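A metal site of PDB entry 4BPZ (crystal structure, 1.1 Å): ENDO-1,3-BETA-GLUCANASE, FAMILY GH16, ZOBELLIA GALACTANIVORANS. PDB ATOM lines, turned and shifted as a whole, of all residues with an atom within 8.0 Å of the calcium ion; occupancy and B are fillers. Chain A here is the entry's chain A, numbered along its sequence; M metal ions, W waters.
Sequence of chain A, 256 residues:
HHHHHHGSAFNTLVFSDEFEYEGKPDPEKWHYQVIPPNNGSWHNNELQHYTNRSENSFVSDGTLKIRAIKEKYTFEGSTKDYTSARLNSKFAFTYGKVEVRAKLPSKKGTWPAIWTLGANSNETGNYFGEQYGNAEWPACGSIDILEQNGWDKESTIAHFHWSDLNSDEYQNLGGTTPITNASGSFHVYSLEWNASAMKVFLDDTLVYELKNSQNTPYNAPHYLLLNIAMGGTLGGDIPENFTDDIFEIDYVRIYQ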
ATOM      1  N   ASP A  17      13.994  -1.627 -21.162  1.00  0.00           N
ATOM      2  CA  ASP A  17      12.922  -1.403 -22.155  1.00  0.00           C
ATOM      3  C   ASP A  17      13.296  -0.077 -22.827  1.00  0.00           C
ATOM      4  O   ASP A  17      13.293   0.970 -22.159  1.00  0.00           O
ATOM      5  CB  ASP A  17      11.487  -1.444 -21.591  1.00  0.00           C
ATOM      6  CG  ASP A  17      10.495  -1.629 -22.711  1.00  0.00           C
ATOM      7  OD1 ASP A  17      10.822  -1.359 -23.881  1.00  0.00           O
ATOM      8  OD2 ASP A  17       9.308  -2.032 -22.338  1.00  0.00           O
ATOM      9  N   GLU A  18      13.629  -0.107 -24.119  1.00  0.00           N
ATOM     10  CA  GLU A  18      13.888   1.076 -24.910  1.00  0.00           C
ATOM     11  C   GLU A  18      12.606   1.691 -25.530  1.00  0.00           C
ATOM     12  O   GLU A  18      12.654   2.743 -26.100  1.00  0.00           O
ATOM     13  CB  GLU A  18      14.865   0.735 -26.055  1.00  0.00           C
ATOM     14  CG  GLU A  18      16.202   0.234 -25.493  1.00  0.00           C
ATOM     15  CD  GLU A  18      16.985   1.225 -24.723  1.00  0.00           C
ATOM     16  OE1 GLU A  18      17.023   2.467 -25.011  1.00  0.00           O
ATOM     17  OE2 GLU A  18      17.693   0.751 -23.799  1.00  0.00           O
ATOM     18  N   PHE A  19      11.494   0.983 -25.371  1.00  0.00           N
ATOM     19  CA  PHE A  19      10.206   1.481 -25.815  1.00  0.00           C
ATOM     20  C   PHE A  19      10.196   1.802 -27.343  1.00  0.00           C
ATOM     21  O   PHE A  19       9.501   2.790 -27.710  1.00  0.00           O
ATOM     22  CB  PHE A  19       9.764   2.685 -24.951  1.00  0.00           C
ATOM     23  CG  PHE A  19       9.503   2.273 -23.540  1.00  0.00           C
ATOM     24  CD1 PHE A  19       8.534   1.329 -23.226  1.00  0.00           C
ATOM     25  CD2 PHE A  19      10.311   2.791 -22.542  1.00  0.00           C
ATOM     26  CE1 PHE A  19       8.326   0.925 -21.896  1.00  0.00           C
ATOM     27  CE2 PHE A  19      10.146   2.371 -21.202  1.00  0.00           C
ATOM     28  CZ  PHE A  19       9.145   1.456 -20.884  1.00  0.00           C
ATOM     29  N   GLU A  20      10.877   1.037 -28.178  1.00  0.00           N
ATOM     30  CA  GLU A  20      10.931   1.345 -29.585  1.00  0.00           C
ATOM     31  C   GLU A  20       9.791   0.664 -30.337  1.00  0.00           C
ATOM     32  O   GLU A  20       9.732   0.839 -31.610  1.00  0.00           O
ATOM     33  CB  GLU A  20      12.370   1.018 -30.098  1.00  0.00           C
ATOM     34  CG  GLU A  20      13.472   1.980 -29.515  1.00  0.00           C
ATOM     35  CD  GLU A  20      13.291   3.556 -29.654  1.00  0.00           C
ATOM     36  OE1 GLU A  20      12.850   3.864 -30.819  1.00  0.00           O
ATOM     37  OE2 GLU A  20      13.602   4.472 -28.667  1.00  0.00           O
ATOM     38  N   TYR A  21       8.877  -0.049 -29.712  1.00  0.00           N
ATOM     39  CA  TYR A  21       7.721  -0.636 -30.296  1.00  0.00           C
ATOM     40  C   TYR A  21       6.436   0.235 -30.166  1.00  0.00           C
ATOM     41  O   TYR A  21       6.535   1.345 -29.619  1.00  0.00           O
ATOM     42  CB  TYR A  21       7.538  -2.004 -29.683  1.00  0.00           C
ATOM     43  CG  TYR A  21       7.427  -1.922 -28.150  1.00  0.00           C
ATOM     44  CD1 TYR A  21       6.186  -1.806 -27.480  1.00  0.00           C
ATOM     45  CD2 TYR A  21       8.538  -2.070 -27.348  1.00  0.00           C
ATOM     46  CE1 TYR A  21       6.099  -1.756 -26.061  1.00  0.00           C
ATOM     47  CE2 TYR A  21       8.489  -1.965 -25.920  1.00  0.00           C
ATOM     48  CZ  TYR A  21       7.306  -1.831 -25.325  1.00  0.00           C
ATOM     49  OH  TYR A  21       7.160  -1.753 -23.906  1.00  0.00           O
ATOM     50  N   VAL A  59       2.758   3.150 -25.754  1.00  0.00           N
ATOM     51  CA  VAL A  59       4.116   3.279 -26.215  1.00  0.00           C
ATOM     52  C   VAL A  59       4.033   3.689 -27.684  1.00  0.00           C
ATOM     53  O   VAL A  59       3.295   3.081 -28.494  1.00  0.00           O
ATOM     54  CB  VAL A  59       4.900   1.967 -26.106  1.00  0.00           C
ATOM     55  CG1 VAL A  59       6.360   2.082 -26.514  1.00  0.00           C
ATOM     56  CG2 VAL A  59       4.832   1.468 -24.628  1.00  0.00           C
ATOM     57  N   SER A  60       4.776   4.726 -28.027  1.00  0.00           N
ATOM     58  CA  SER A  60       4.743   5.206 -29.421  1.00  0.00           C
ATOM     59  C   SER A  60       5.931   6.074 -29.615  1.00  0.00           C
ATOM     60  O   SER A  60       6.463   6.709 -28.665  1.00  0.00           O
ATOM     61  CB  SER A  60       3.507   6.062 -29.725  1.00  0.00           C
ATOM     62  OG  SER A  60       3.385   7.194 -28.858  1.00  0.00           O
ATOM     63  N   ASP A  61       6.414   6.146 -30.855  1.00  0.00           N
ATOM     64  CA  ASP A  61       7.447   7.101 -31.183  1.00  0.00           C
ATOM     65  C   ASP A  61       8.738   7.000 -30.299  1.00  0.00           C
ATOM     66  O   ASP A  61       9.328   8.061 -29.977  1.00  0.00           O
ATOM     67  CB  ASP A  61       6.796   8.525 -31.179  1.00  0.00           C
ATOM     68  CG  ASP A  61       7.661   9.654 -31.755  1.00  0.00           C
ATOM     69  OD1 ASP A  61       8.435   9.411 -32.716  1.00  0.00           O
ATOM     70  OD2 ASP A  61       7.416  10.845 -31.311  1.00  0.00           O
ATOM     71  N   GLY A  62       9.075   5.803 -29.848  1.00  0.00           N
ATOM     72  CA  GLY A  62      10.245   5.547 -29.038  1.00  0.00           C
ATOM     73  C   GLY A  62      10.138   5.824 -27.558  1.00  0.00           C
ATOM     74  O   GLY A  62      11.127   5.632 -26.830  1.00  0.00           O
ATOM     75  N   THR A  63       8.947   6.131 -27.012  1.00  0.00           N
ATOM     76  CA  THR A  63       8.810   6.407 -25.623  1.00  0.00           C
ATOM     77  C   THR A  63       7.521   5.832 -25.064  1.00  0.00           C
ATOM     78  O   THR A  63       6.469   5.691 -25.750  1.00  0.00           O
ATOM     79  CB  THR A  63       8.823   7.937 -25.295  1.00  0.00           C
ATOM     80  OG1 THR A  63       7.676   8.553 -25.852  1.00  0.00           O
ATOM     81  CG2 THR A  63       9.972   8.666 -25.810  1.00  0.00           C
ATOM     82  N   LEU A  64       7.570   5.477 -23.765  1.00  0.00           N
ATOM     83  CA  LEU A  64       6.381   5.157 -22.987  1.00  0.00           C
ATOM     84  C   LEU A  64       5.773   6.447 -22.506  1.00  0.00           C
ATOM     85  O   LEU A  64       6.464   7.352 -22.029  1.00  0.00           O
ATOM     86  CB  LEU A  64       6.858   4.316 -21.741  1.00  0.00           C
ATOM     87  CG  LEU A  64       5.794   4.150 -20.647  1.00  0.00           C
ATOM     88  CD1 LEU A  64       4.641   3.271 -21.108  1.00  0.00           C
ATOM     89  CD2 LEU A  64       6.469   3.558 -19.436  1.00  0.00           C
ATOM     90  N   ARG A 101      15.367   7.586 -18.308  1.00  0.00           N
ATOM     91  CA  ARG A 101      15.453   8.909 -18.962  1.00  0.00           C
ATOM     92  C   ARG A 101      14.001   9.346 -19.252  1.00  0.00           C
ATOM     93  O   ARG A 101      13.237   8.591 -19.877  1.00  0.00           O
ATOM     94  CB  ARG A 101      16.221   8.766 -20.278  1.00  0.00           C
ATOM     95  CG  ARG A 101      16.366  10.098 -21.006  1.00  0.00           C
ATOM     96  CD  ARG A 101      17.384   9.954 -22.155  1.00  0.00           C
ATOM     97  NE  ARG A 101      17.674  11.266 -22.719  1.00  0.00           N
ATOM     98  CZ  ARG A 101      17.270  11.673 -23.913  1.00  0.00           C
ATOM     99  NH1 ARG A 101      16.440  10.969 -24.667  1.00  0.00           N
ATOM    100  NH2 ARG A 101      17.599  12.895 -24.331  1.00  0.00           N
ATOM    101  N   PHE A 186      14.429  16.009 -21.493  1.00  0.00           N
ATOM    102  CA  PHE A 186      14.759  14.743 -20.826  1.00  0.00           C
ATOM    103  C   PHE A 186      15.883  14.938 -19.798  1.00  0.00           C
ATOM    104  O   PHE A 186      16.860  15.619 -20.052  1.00  0.00           O
ATOM    105  CB  PHE A 186      15.181  13.689 -21.853  1.00  0.00           C
ATOM    106  CG  PHE A 186      14.096  13.085 -22.642  1.00  0.00           C
ATOM    107  CD1 PHE A 186      13.178  12.195 -22.033  1.00  0.00           C
ATOM    108  CD2 PHE A 186      13.889  13.449 -24.003  1.00  0.00           C
ATOM    109  CE1 PHE A 186      12.149  11.652 -22.739  1.00  0.00           C
ATOM    110  CE2 PHE A 186      12.829  12.853 -24.710  1.00  0.00           C
ATOM    111  CZ  PHE A 186      11.916  12.011 -24.066  1.00  0.00           C
ATOM    112  N   ILE A 249       8.675   8.476 -20.771  1.00  0.00           N
ATOM    113  CA  ILE A 249       9.902   7.732 -20.411  1.00  0.00           C
ATOM    114  C   ILE A 249      10.527   7.172 -21.681  1.00  0.00           C
ATOM    115  O   ILE A 249       9.954   6.365 -22.414  1.00  0.00           O
ATOM    116  CB  ILE A 249       9.517   6.599 -19.393  1.00  0.00           C
ATOM    117  CG1 ILE A 249       9.059   7.274 -18.114  1.00  0.00           C
ATOM    118  CG2 ILE A 249      10.717   5.711 -19.183  1.00  0.00           C
ATOM    119  CD1 ILE A 249       8.380   6.351 -17.231  1.00  0.00           C
ATOM    120  N   ASP A 250      11.737   7.622 -21.979  1.00  0.00           N
ATOM    121  CA  ASP A 250      12.480   7.156 -23.170  1.00  0.00           C
ATOM    122  C   ASP A 250      12.986   5.731 -22.984  1.00  0.00           C
ATOM    123  O   ASP A 250      12.924   4.906 -23.902  1.00  0.00           O
ATOM    124  CB  ASP A 250      13.614   8.164 -23.421  1.00  0.00           C
ATOM    125  CG  ASP A 250      14.383   7.849 -24.682  1.00  0.00           C
ATOM    126  OD1 ASP A 250      13.843   7.215 -25.626  1.00  0.00           O
ATOM    127  OD2 ASP A 250      15.562   8.276 -24.732  1.00  0.00           O
ATOM    128  N   TYR A 251      13.505   5.402 -21.796  1.00  0.00           N
ATOM    129  CA  TYR A 251      13.983   4.075 -21.576  1.00  0.00           C
ATOM    130  C   TYR A 251      14.093   3.833 -20.042  1.00  0.00           C
ATOM    131  O   TYR A 251      14.207   4.774 -19.271  1.00  0.00           O
ATOM    132  CB  TYR A 251      15.394   3.808 -22.185  1.00  0.00           C
ATOM    133  CG  TYR A 251      16.500   4.724 -21.825  1.00  0.00           C
ATOM    134  CD1 TYR A 251      17.106   4.692 -20.559  1.00  0.00           C
ATOM    135  CD2 TYR A 251      16.997   5.668 -22.753  1.00  0.00           C
ATOM    136  CE1 TYR A 251      18.199   5.477 -20.234  1.00  0.00           C
ATOM    137  CE2 TYR A 251      18.068   6.479 -22.444  1.00  0.00           C
ATOM    138  CZ  TYR A 251      18.683   6.390 -21.209  1.00  0.00           C
ATOM    139  OH  TYR A 251      19.704   7.235 -20.921  1.00  0.00           O
ATOM    140  N   VAL A 252      14.107   2.545 -19.744  1.00  0.00           N
ATOM    141  CA  VAL A 252      14.522   2.019 -18.387  1.00  0.00           C
ATOM    142  C   VAL A 252      15.654   1.068 -18.662  1.00  0.00           C
ATOM    143  O   VAL A 252      15.475   0.159 -19.507  1.00  0.00           O
ATOM    144  CB  VAL A 252      13.347   1.278 -17.721  1.00  0.00           C
ATOM    145  CG1 VAL A 252      13.795   0.610 -16.418  1.00  0.00           C
ATOM    146  CG2 VAL A 252      12.196   2.243 -17.473  1.00  0.00           C
ATOM    147  N   ARG A 253      16.775   1.225 -17.969  1.00  0.00           N
ATOM    148  CA  ARG A 253      17.895   0.274 -18.093  1.00  0.00           C
ATOM    149  C   ARG A 253      18.345  -0.094 -16.675  1.00  0.00           C
ATOM    150  O   ARG A 253      18.477   0.773 -15.821  1.00  0.00           O
ATOM    151  CB  ARG A 253      19.063   0.893 -18.853  1.00  0.00           C
ATOM    152  CG  ARG A 253      18.741   1.259 -20.318  1.00  0.00           C
ATOM    153  CD  ARG A 253      19.806   2.097 -20.925  1.00  0.00           C
ATOM    154  NE  ARG A 253      19.422   2.450 -22.287  1.00  0.00           N
ATOM    155  CZ  ARG A 253      19.986   3.426 -22.979  1.00  0.00           C
ATOM    156  NH1 ARG A 253      21.001   4.090 -22.525  1.00  0.00           N
ATOM    157  NH2 ARG A 253      19.468   3.689 -24.190  1.00  0.00           N
HETATM  158 CA    CA M   1      13.235   5.027 -26.297  1.00  0.00          CA
HETATM  159  O   HOH W   1      15.551   4.463 -26.126  1.00  0.00           O
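The side-chain carboxylate (OE1) of Glu 18 is in salt-bridge range of the guanidinium group (NH2) of Arg 253. The side-chain carboxylate of Asp 250 lies within salt-bridge range of the guanidinium group of Arg 101 (2.8 Å).
The nearest printed residue that does not touch the calcium ion is Phe 19 (4.4 Å).
The calcium ion is bound by the backbone carbonyl oxygen (O) of Gly 62 (2.3 Å). O of Glu 18 is bound to the calcium ion (2.4 Å). The calcium ion is bound by OD1 of Asp 250, at 2.4 Å. The calcium ion is bound by water W1. The calcium ion is bound by the backbone carbonyl oxygen (O) of Asp 250. OE2 of Glu 20 binds the calcium ion, 2.5 Å away.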
